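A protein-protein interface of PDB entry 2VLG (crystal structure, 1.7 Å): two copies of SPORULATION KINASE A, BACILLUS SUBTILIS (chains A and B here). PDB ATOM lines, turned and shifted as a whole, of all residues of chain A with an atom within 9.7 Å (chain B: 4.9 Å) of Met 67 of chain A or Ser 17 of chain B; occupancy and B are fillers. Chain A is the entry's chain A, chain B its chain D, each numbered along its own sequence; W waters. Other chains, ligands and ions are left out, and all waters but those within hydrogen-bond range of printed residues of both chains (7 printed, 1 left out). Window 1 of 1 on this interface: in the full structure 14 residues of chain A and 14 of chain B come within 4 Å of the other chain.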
ATOM      1  N   LEU A  55     -13.400 -23.394 -29.030  1.00  0.00           N
ATOM      2  CA  LEU A  55     -12.822 -22.089 -28.749  1.00  0.00           C
ATOM      3  C   LEU A  55     -11.318 -22.156 -28.442  1.00  0.00           C
ATOM      4  O   LEU A  55     -10.497 -21.431 -29.080  1.00  0.00           O
ATOM      5  CB  LEU A  55     -13.591 -21.433 -27.593  1.00  0.00           C
ATOM      6  CG  LEU A  55     -13.013 -20.236 -26.860  1.00  0.00           C
ATOM      7  CD1 LEU A  55     -13.428 -18.931 -27.587  1.00  0.00           C
ATOM      8  CD2 LEU A  55     -13.512 -20.231 -25.438  1.00  0.00           C
ATOM      9  N   TYR A  59      -8.125 -21.187 -30.866  1.00  0.00           N
ATOM     10  CA  TYR A  59      -7.241 -20.127 -30.400  1.00  0.00           C
ATOM     11  C   TYR A  59      -5.769 -20.496 -30.568  1.00  0.00           C
ATOM     12  O   TYR A  59      -4.964 -19.710 -31.097  1.00  0.00           O
ATOM     13  CB  TYR A  59      -7.510 -19.838 -28.914  1.00  0.00           C
ATOM     14  CG  TYR A  59      -6.757 -18.663 -28.400  1.00  0.00           C
ATOM     15  CD1 TYR A  59      -7.286 -17.379 -28.523  1.00  0.00           C
ATOM     16  CD2 TYR A  59      -5.487 -18.810 -27.783  1.00  0.00           C
ATOM     17  CE1 TYR A  59      -6.590 -16.299 -28.069  1.00  0.00           C
ATOM     18  CE2 TYR A  59      -4.808 -17.716 -27.296  1.00  0.00           C
ATOM     19  CZ  TYR A  59      -5.360 -16.460 -27.480  1.00  0.00           C
ATOM     20  OH  TYR A  59      -4.685 -15.360 -27.013  1.00  0.00           O
ATOM     21  N   PHE A  60      -5.420 -21.706 -30.136  1.00  0.00           N
ATOM     22  CA  PHE A  60      -4.015 -22.053 -30.046  1.00  0.00           C
ATOM     23  C   PHE A  60      -3.450 -22.576 -31.340  1.00  0.00           C
ATOM     24  O   PHE A  60      -2.225 -22.617 -31.486  1.00  0.00           O
ATOM     25  CB  PHE A  60      -3.717 -22.959 -28.839  1.00  0.00           C
ATOM     26  CG  PHE A  60      -3.705 -22.209 -27.536  1.00  0.00           C
ATOM     27  CD1 PHE A  60      -2.708 -21.266 -27.262  1.00  0.00           C
ATOM     28  CD2 PHE A  60      -4.730 -22.389 -26.613  1.00  0.00           C
ATOM     29  CE1 PHE A  60      -2.709 -20.517 -26.063  1.00  0.00           C
ATOM     30  CE2 PHE A  60      -4.757 -21.660 -25.451  1.00  0.00           C
ATOM     31  CZ  PHE A  60      -3.740 -20.713 -25.165  1.00  0.00           C
ATOM     32  N   ASN A  62      -4.233 -20.888 -34.255  1.00  0.00           N
ATOM     33  CA  ASN A  62      -4.033 -19.613 -34.934  1.00  0.00           C
ATOM     34  C   ASN A  62      -2.754 -18.889 -34.601  1.00  0.00           C
ATOM     35  O   ASN A  62      -2.300 -18.949 -33.490  1.00  0.00           O
ATOM     36  CB  ASN A  62      -5.265 -18.744 -34.680  1.00  0.00           C
ATOM     37  CG  ASN A  62      -6.444 -19.171 -35.569  1.00  0.00           C
ATOM     38  OD1 ASN A  62      -6.254 -19.529 -36.724  1.00  0.00           O
ATOM     39  ND2 ASN A  62      -7.647 -19.138 -35.026  1.00  0.00           N
ATOM     40  N   GLU A  63      -2.175 -18.195 -35.578  1.00  0.00           N
ATOM     41  CA  GLU A  63      -0.868 -17.536 -35.382  1.00  0.00           C
ATOM     42  C   GLU A  63      -1.000 -16.180 -34.731  1.00  0.00           C
ATOM     43  O   GLU A  63      -0.127 -15.756 -33.954  1.00  0.00           O
ATOM     44  CB  GLU A  63      -0.112 -17.360 -36.711  1.00  0.00           C
ATOM     45  CG  GLU A  63       0.143 -18.664 -37.491  1.00  0.00           C
ATOM     46  CD  GLU A  63       1.223 -19.552 -36.882  1.00  0.00           C
ATOM     47  OE1 GLU A  63       2.358 -19.547 -37.412  1.00  0.00           O
ATOM     48  OE2 GLU A  63       0.938 -20.261 -35.891  1.00  0.00           O
ATOM     49  N   HIS A  64      -2.077 -15.475 -35.076  1.00  0.00           N
ATOM     50  CA  HIS A  64      -2.157 -14.072 -34.692  1.00  0.00           C
ATOM     51  C   HIS A  64      -2.964 -13.953 -33.452  1.00  0.00           C
ATOM     52  O   HIS A  64      -4.034 -14.511 -33.394  1.00  0.00           O
ATOM     53  CB  HIS A  64      -2.815 -13.278 -35.811  1.00  0.00           C
ATOM     54  CG  HIS A  64      -1.941 -13.127 -37.011  1.00  0.00           C
ATOM     55  ND1 HIS A  64      -0.945 -12.173 -37.085  1.00  0.00           N
ATOM     56  CD2 HIS A  64      -1.878 -13.831 -38.164  1.00  0.00           C
ATOM     57  CE1 HIS A  64      -0.306 -12.293 -38.235  1.00  0.00           C
ATOM     58  NE2 HIS A  64      -0.852 -13.293 -38.908  1.00  0.00           N
ATOM     59  N   HIS A  65      -2.467 -13.218 -32.465  1.00  0.00           N
ATOM     60  CA  HIS A  65      -3.239 -13.023 -31.212  1.00  0.00           C
ATOM     61  C   HIS A  65      -3.141 -11.600 -30.749  1.00  0.00           C
ATOM     62  O   HIS A  65      -2.186 -10.906 -31.113  1.00  0.00           O
ATOM     63  CB  HIS A  65      -2.706 -13.933 -30.093  1.00  0.00           C
ATOM     64  CG  HIS A  65      -2.824 -15.384 -30.417  1.00  0.00           C
ATOM     65  ND1 HIS A  65      -1.733 -16.146 -30.765  1.00  0.00           N
ATOM     66  CD2 HIS A  65      -3.893 -16.203 -30.469  1.00  0.00           C
ATOM     67  CE1 HIS A  65      -2.122 -17.384 -30.990  1.00  0.00           C
ATOM     68  NE2 HIS A  65      -3.423 -17.448 -30.815  1.00  0.00           N
ATOM     69  N   LEU A  66      -4.129 -11.154 -29.989  1.00  0.00           N
ATOM     70  CA  LEU A  66      -3.983  -9.939 -29.232  1.00  0.00           C
ATOM     71  C   LEU A  66      -4.597 -10.185 -27.874  1.00  0.00           C
ATOM     72  O   LEU A  66      -3.904 -10.182 -26.876  1.00  0.00           O
ATOM     73  CB  LEU A  66      -4.616  -8.719 -29.943  1.00  0.00           C
ATOM     74  CG  LEU A  66      -4.503  -7.389 -29.222  1.00  0.00           C
ATOM     75  CD1 LEU A  66      -3.059  -7.057 -28.935  1.00  0.00           C
ATOM     76  CD2 LEU A  66      -5.123  -6.284 -30.081  1.00  0.00           C
ATOM     77  N   MET A  67      -5.881 -10.490 -27.832  1.00  0.00           N
ATOM     78  CA  MET A  67      -6.559 -10.743 -26.549  1.00  0.00           C
ATOM     79  C   MET A  67      -6.190 -12.136 -26.084  1.00  0.00           C
ATOM     80  O   MET A  67      -5.959 -13.005 -26.902  1.00  0.00           O
ATOM     81  CB  MET A  67      -8.049 -10.680 -26.736  1.00  0.00           C
ATOM     82  CG  MET A  67      -8.395  -9.280 -27.217  1.00  0.00           C
ATOM     83  SD  MET A  67     -10.144  -8.950 -27.073  1.00  0.00           S
ATOM     84  CE  MET A  67     -10.272  -8.704 -25.290  1.00  0.00           C
ATOM     85  N   PRO A  68      -6.163 -12.347 -24.776  1.00  0.00           N
ATOM     86  CA  PRO A  68      -6.064 -13.723 -24.225  1.00  0.00           C
ATOM     87  C   PRO A  68      -7.258 -14.578 -24.547  1.00  0.00           C
ATOM     88  O   PRO A  68      -8.303 -14.060 -25.040  1.00  0.00           O
ATOM     89  CB  PRO A  68      -6.072 -13.508 -22.705  1.00  0.00           C
ATOM     90  CG  PRO A  68      -6.470 -12.108 -22.490  1.00  0.00           C
ATOM     91  CD  PRO A  68      -6.140 -11.327 -23.731  1.00  0.00           C
ATOM     92  N   CYS A  69      -7.157 -15.868 -24.217  1.00  0.00           N
ATOM     93  CA  CYS A  69      -8.286 -16.802 -24.464  1.00  0.00           C
ATOM     94  C   CYS A  69      -8.815 -16.986 -23.082  1.00  0.00           C
ATOM     95  O   CYS A  69      -8.051 -17.366 -22.240  1.00  0.00           O
ATOM     96  CB  CYS A  69      -7.781 -18.181 -24.926  1.00  0.00           C
ATOM     97  SG  CYS A  69      -9.096 -19.364 -25.476  1.00  0.00           S
ATOM     98  N   THR A  70     -10.125 -16.801 -22.889  1.00  0.00           N
ATOM     99  CA  THR A  70     -10.797 -16.965 -21.647  1.00  0.00           C
ATOM    100  C   THR A  70     -11.638 -18.213 -21.763  1.00  0.00           C
ATOM    101  O   THR A  70     -12.465 -18.319 -22.674  1.00  0.00           O
ATOM    102  CB  THR A  70     -11.712 -15.719 -21.380  1.00  0.00           C
ATOM    103  OG1 THR A  70     -10.837 -14.562 -21.360  1.00  0.00           O
ATOM    104  CG2 THR A  70     -12.379 -15.827 -20.029  1.00  0.00           C
ATOM    105  N   GLU A  84      -7.582 -17.196 -18.039  1.00  0.00           N
ATOM    106  CA  GLU A  84      -7.202 -16.627 -19.334  1.00  0.00           C
ATOM    107  C   GLU A  84      -5.801 -17.072 -19.635  1.00  0.00           C
ATOM    108  O   GLU A  84      -4.960 -17.098 -18.743  1.00  0.00           O
ATOM    109  CB  GLU A  84      -7.302 -15.108 -19.333  1.00  0.00           C
ATOM    110  CG  GLU A  84      -6.384 -14.420 -18.377  1.00  0.00           C
ATOM    111  CD  GLU A  84      -6.477 -12.948 -18.570  1.00  0.00           C
ATOM    112  OE1 GLU A  84      -7.562 -12.403 -18.281  1.00  0.00           O
ATOM    113  OE2 GLU A  84      -5.481 -12.360 -19.006  1.00  0.00           O
ATOM    114  N   ALA A  85      -5.540 -17.338 -20.912  1.00  0.00           N
ATOM    115  CA  ALA A  85      -4.251 -17.817 -21.350  1.00  0.00           C
ATOM    116  C   ALA A  85      -3.795 -17.022 -22.540  1.00  0.00           C
ATOM    117  O   ALA A  85      -4.618 -16.587 -23.374  1.00  0.00           O
ATOM    118  CB  ALA A  85      -4.388 -19.302 -21.760  1.00  0.00           C
ATOM    119  N   ALA A  86      -2.482 -16.877 -22.670  1.00  0.00           N
ATOM    120  CA  ALA A  86      -1.893 -16.139 -23.793  1.00  0.00           C
ATOM    121  C   ALA A  86      -0.643 -16.882 -24.231  1.00  0.00           C
ATOM    122  O   ALA A  86       0.032 -17.486 -23.384  1.00  0.00           O
ATOM    123  CB  ALA A  86      -1.520 -14.767 -23.338  1.00  0.00           C
ATOM    124  N   VAL A  87      -0.376 -16.893 -25.537  1.00  0.00           N
ATOM    125  CA  VAL A  87       0.883 -17.394 -26.082  1.00  0.00           C
ATOM    126  C   VAL A  87       2.015 -16.503 -25.572  1.00  0.00           C
ATOM    127  O   VAL A  87       2.014 -15.278 -25.843  1.00  0.00           O
ATOM    128  CB  VAL A  87       0.838 -17.480 -27.628  1.00  0.00           C
ATOM    129  CG1 VAL A  87       2.152 -17.924 -28.196  1.00  0.00           C
ATOM    130  CG2 VAL A  87      -0.245 -18.450 -28.059  1.00  0.00           C
ATOM    131  N   LYS A 104       1.126 -18.854 -21.076  1.00  0.00           N
ATOM    132  CA  LYS A 104       1.021 -18.468 -19.676  1.00  0.00           C
ATOM    133  C   LYS A 104      -0.463 -18.352 -19.427  1.00  0.00           C
ATOM    134  O   LYS A 104      -1.231 -17.980 -20.325  1.00  0.00           O
ATOM    135  CB  LYS A 104       1.709 -17.160 -19.372  1.00  0.00           C
ATOM    136  CG  LYS A 104       1.280 -15.968 -20.237  1.00  0.00           C
ATOM    137  CD  LYS A 104       1.895 -14.680 -19.737  1.00  0.00           C
ATOM    138  CE  LYS A 104       1.545 -13.636 -20.735  1.00  0.00           C
ATOM    139  NZ  LYS A 104       2.038 -12.263 -20.365  1.00  0.00           N
ATOM    140  N   LEU B  15     -10.725  -3.506 -33.569  1.00  0.00           N
ATOM    141  CA  LEU B  15      -9.902  -4.681 -33.831  1.00  0.00           C
ATOM    142  C   LEU B  15     -10.750  -5.907 -33.526  1.00  0.00           C
ATOM    143  O   LEU B  15     -11.525  -5.920 -32.582  1.00  0.00           O
ATOM    144  CB  LEU B  15      -8.635  -4.720 -32.919  1.00  0.00           C
ATOM    145  CG  LEU B  15      -7.820  -3.435 -32.852  1.00  0.00           C
ATOM    146  CD1 LEU B  15      -6.564  -3.645 -31.980  1.00  0.00           C
ATOM    147  CD2 LEU B  15      -7.385  -3.060 -34.273  1.00  0.00           C
ATOM    148  N   ALA B  16     -10.551  -6.962 -34.293  1.00  0.00           N
ATOM    149  CA  ALA B  16     -11.010  -8.284 -33.893  1.00  0.00           C
ATOM    150  C   ALA B  16     -10.204  -8.699 -32.660  1.00  0.00           C
ATOM    151  O   ALA B  16      -9.162  -8.120 -32.358  1.00  0.00           O
ATOM    152  CB  ALA B  16     -10.783  -9.277 -35.037  1.00  0.00           C
ATOM    153  N   SER B  17     -10.678  -9.707 -31.942  1.00  0.00           N
ATOM    154  CA  SER B  17      -9.954 -10.133 -30.734  1.00  0.00           C
ATOM    155  C   SER B  17      -8.510 -10.609 -31.012  1.00  0.00           C
ATOM    156  O   SER B  17      -7.654 -10.613 -30.110  1.00  0.00           O
ATOM    157  CB  SER B  17     -10.755 -11.241 -30.016  1.00  0.00           C
ATOM    158  OG  SER B  17     -10.968 -12.314 -30.919  1.00  0.00           O
ATOM    159  N   ASN B  18      -8.251 -11.002 -32.253  1.00  0.00           N
ATOM    160  CA  ASN B  18      -6.922 -11.464 -32.651  1.00  0.00           C
ATOM    161  C   ASN B  18      -6.028 -10.366 -33.184  1.00  0.00           C
ATOM    162  O   ASN B  18      -4.937 -10.662 -33.732  1.00  0.00           O
ATOM    163  CB  ASN B  18      -7.022 -12.560 -33.716  1.00  0.00           C
ATOM    164  CG  ASN B  18      -7.638 -12.062 -35.019  1.00  0.00           C
ATOM    165  OD1 ASN B  18      -7.995 -10.883 -35.173  1.00  0.00           O
ATOM    166  ND2 ASN B  18      -7.713 -12.967 -35.994  1.00  0.00           N
ATOM    167  N   GLY B  19      -6.492  -9.129 -33.098  1.00  0.00           N
ATOM    168  CA  GLY B  19      -5.667  -7.956 -33.493  1.00  0.00           C
ATOM    169  C   GLY B  19      -5.858  -7.473 -34.931  1.00  0.00           C
ATOM    170  O   GLY B  19      -5.257  -6.489 -35.319  1.00  0.00           O
ATOM    171  N   GLU B  57       0.141  -6.428 -26.483  1.00  0.00           N
ATOM    172  CA  GLU B  57      -0.497  -7.701 -26.141  1.00  0.00           C
ATOM    173  C   GLU B  57      -0.543  -7.831 -24.637  1.00  0.00           C
ATOM    174  O   GLU B  57      -1.492  -8.403 -24.094  1.00  0.00           O
ATOM    175  CB  GLU B  57       0.137  -8.953 -26.824  1.00  0.00           C
ATOM    176  CG  GLU B  57      -0.845 -10.165 -26.665  1.00  0.00           C
ATOM    177  CD  GLU B  57      -0.433 -11.471 -27.349  1.00  0.00           C
ATOM    178  OE1 GLU B  57       0.571 -11.436 -28.104  1.00  0.00           O
ATOM    179  OE2 GLU B  57      -1.149 -12.518 -27.118  1.00  0.00           O
ATOM    180  N   PHE B  60      -3.687  -6.368 -22.807  1.00  0.00           N
ATOM    181  CA  PHE B  60      -4.912  -7.161 -22.795  1.00  0.00           C
ATOM    182  C   PHE B  60      -4.853  -8.377 -21.903  1.00  0.00           C
ATOM    183  O   PHE B  60      -5.855  -9.062 -21.757  1.00  0.00           O
ATOM    184  CB  PHE B  60      -5.256  -7.550 -24.222  1.00  0.00           C
ATOM    185  CG  PHE B  60      -5.660  -6.393 -25.050  1.00  0.00           C
ATOM    186  CD1 PHE B  60      -6.989  -5.929 -25.025  1.00  0.00           C
ATOM    187  CD2 PHE B  60      -4.739  -5.709 -25.785  1.00  0.00           C
ATOM    188  CE1 PHE B  60      -7.357  -4.837 -25.761  1.00  0.00           C
ATOM    189  CE2 PHE B  60      -5.103  -4.577 -26.520  1.00  0.00           C
ATOM    190  CZ  PHE B  60      -6.419  -4.153 -26.517  1.00  0.00           C
ATOM    191  N   ILE B  89     -13.943  -2.886 -24.586  1.00  0.00           N
ATOM    192  CA  ILE B  89     -14.235  -4.193 -25.138  1.00  0.00           C
ATOM    193  C   ILE B  89     -15.740  -4.379 -25.243  1.00  0.00           C
ATOM    194  O   ILE B  89     -16.503  -4.189 -24.262  1.00  0.00           O
ATOM    195  CB  ILE B  89     -13.594  -5.386 -24.279  1.00  0.00           C
ATOM    196  CG1 ILE B  89     -12.092  -5.209 -24.124  1.00  0.00           C
ATOM    197  CG2 ILE B  89     -13.871  -6.732 -24.941  1.00  0.00           C
ATOM    198  CD1 ILE B  89     -11.354  -4.999 -25.396  1.00  0.00           C
ATOM    199  N   ARG B  99     -15.398 -11.109 -28.786  1.00  0.00           N
ATOM    200  CA  ARG B  99     -14.958  -9.822 -28.191  1.00  0.00           C
ATOM    201  C   ARG B  99     -14.438  -8.960 -29.312  1.00  0.00           C
ATOM    202  O   ARG B  99     -13.761  -9.449 -30.216  1.00  0.00           O
ATOM    203  CB  ARG B  99     -13.875 -10.007 -27.122  1.00  0.00           C
ATOM    204  CG  ARG B  99     -14.400 -10.799 -25.900  1.00  0.00           C
ATOM    205  CD  ARG B  99     -13.295 -11.074 -24.893  1.00  0.00           C
ATOM    206  NE  ARG B  99     -13.843 -11.775 -23.736  1.00  0.00           N
ATOM    207  CZ  ARG B  99     -14.071 -13.089 -23.741  1.00  0.00           C
ATOM    208  NH1 ARG B  99     -13.785 -13.796 -24.832  1.00  0.00           N
ATOM    209  NH2 ARG B  99     -14.608 -13.715 -22.694  1.00  0.00           N
ATOM    210  N   ILE B 101     -12.629  -5.060 -30.055  1.00  0.00           N
ATOM    211  CA  ILE B 101     -11.914  -4.010 -29.366  1.00  0.00           C
ATOM    212  C   ILE B 101     -12.192  -2.694 -30.076  1.00  0.00           C
ATOM    213  O   ILE B 101     -11.911  -2.560 -31.264  1.00  0.00           O
ATOM    214  CB  ILE B 101     -10.389  -4.266 -29.383  1.00  0.00           C
ATOM    215  CG1 ILE B 101     -10.038  -5.588 -28.666  1.00  0.00           C
ATOM    216  CG2 ILE B 101      -9.633  -3.057 -28.725  1.00  0.00           C
ATOM    217  CD1 ILE B 101      -8.583  -6.068 -29.060  1.00  0.00           C
HETATM  218  O   HOH W   1      -2.853 -10.690 -24.106  1.00  0.00           O
HETATM  219  O   HOH W   2      -6.077 -13.378 -29.786  1.00  0.00           O
HETATM  220  O   HOH W   3      -2.309  -9.884 -33.827  1.00  0.00           O
HETATM  221  O   HOH W   4       1.288 -12.884 -24.706  1.00  0.00           O
HETATM  222  O   HOH W   5     -10.520 -13.320 -23.738  1.00  0.00           O
HETATM  223  O   HOH W   6       1.527 -13.837 -28.207  1.00  0.00           O
HETATM  224  O   HOH W   7      -1.841 -15.187 -27.245  1.00  0.00           O
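Water W1 lies within hydrogen-bond range of the backbone carbonyl oxygen (O) of Glu 57 of chain B (2.7 Å) and the backbone carbonyl oxygen (O) of Leu 66 of chain A (3.0 Å).
Water W5 lies within hydrogen-bond range of O of Pro 68 of chain A (2.7 Å), OG1 of Thr 70 of chain A (2.7 Å) and NH1 of Arg 99 of chain B (3.5 Å).
Water W3 lies within hydrogen-bond range of the backbone carbonyl oxygen (O) of Asn 18 of chain B (2.7 Å) and the backbone carbonyl oxygen (O) of His 65 of chain A (2.9 Å).
Water W4 lies within hydrogen-bond range of O of Val 87 of chain A (2.7 Å) and OE2 of Glu 57 of chain B (3.4 Å).
Water W7 lies within hydrogen-bond range of OE2 of Glu 57 of chain B, N of Val 87 of chain A and OH of Tyr 59 of chain A.
Water W2 lies within hydrogen-bond range of the backbone carbonyl oxygen of Met 67 of chain A (2.9 Å), the backbone NH of Leu 66 of chain A (3.0 Å) and the backbone carbonyl oxygen of Ser 17 of chain B (3.2 Å).
Position printed for both chains: 60.
Of the 10 printed residues of chain B, 9 touch a printed residue of chain A.
Printed residues of chain B that touch a printed residue of chain A: Leu 15, Ser 17, Asn 18, Gly 19, Glu 57, Phe 60, Ile 89, Arg 99 and Ile 101.
Among the printed residues, 16 pairs touch across the chains.
Among the printed residues, no Asp or Glu carboxylate lies within 4 Å of a Lys or Arg side-chain nitrogen of the other chain.
Met 67 of chain A touches just these residues of chain B: Ser 17 (2.9 Å), Ile 89 (3.9 Å), Arg 99 (3.9 Å) and Ile 101 (3.7 Å).
No residue of chain A comes within 4 Å of Ala 16 of chain B.
Of the printed residues of chain B, Pro 68 of chain A touches Phe 60.
Of the printed residues of chain B, Leu 66 of chain A touches Leu 15 (3.6 Å), Ser 17 (3.6 Å), Asn 18 (3.8 Å), Gly 19 (3.7 Å), Glu 57 (3.1 Å), Phe 60 (3.8 Å) and Ile 101 (3.6 Å).
Of the printed residues of chain A, Leu 15 of chain B touches Leu 66.
Asn 62 of chain A touches none of the printed residues of chain B.
Lys 104 of chain A touches none of the printed residues of chain B.
The nearest residue of chain B that does not touch Met 67 of chain A is Phe 60 of chain B (4.2 Å).
The backbone NH (N) of Met 67 of chain A lies within hydrogen-bond range of the backbone carbonyl oxygen (O) of Ser 17 of chain B (2.9 Å).
His 65 of chain A touches Asn 18 of chain B (C to O, 3.6 Å).
Glu 57 of chain B touches His 65 of chain A.
Leu 66 of chain A touches Ser 17 of chain B (N to O, 3.6 Å).
CG of Glu 57 of chain B touches O of Leu 66 of chain A, at 3.1 Å.
Phe 60 of chain B touches Leu 66 of chain A.
CD1 of Ile 101 of chain B touches CD2 of Leu 66 of chain A, 3.6 Å away.
Met 67 of chain A touches Arg 99 of chain B (CE to CD, 3.9 Å).
Met 67 of chain A touches Ile 101 of chain B.
Pro 68 of chain A touches Phe 60 of chain B.
Thr 70 of chain A touches Arg 99 of chain B.
NE2 of His 65 of chain A lies within hydrogen-bond range of O of Tyr 59 of chain A, 2.8 Å away.
N of Leu 15 of chain B is in hydrogen-bond range of O of Ile 101 of chain B, 2.8 Å away.
The side-chain hydroxyl (OH) of Tyr 59 of chain A lies within hydrogen-bond range of the backbone carbonyl oxygen (O) of Met 67 of chain A, 2.7 Å away.
NE2 of His 65 of chain A lies close to O of Asn 62 of chain A (3.3 Å).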
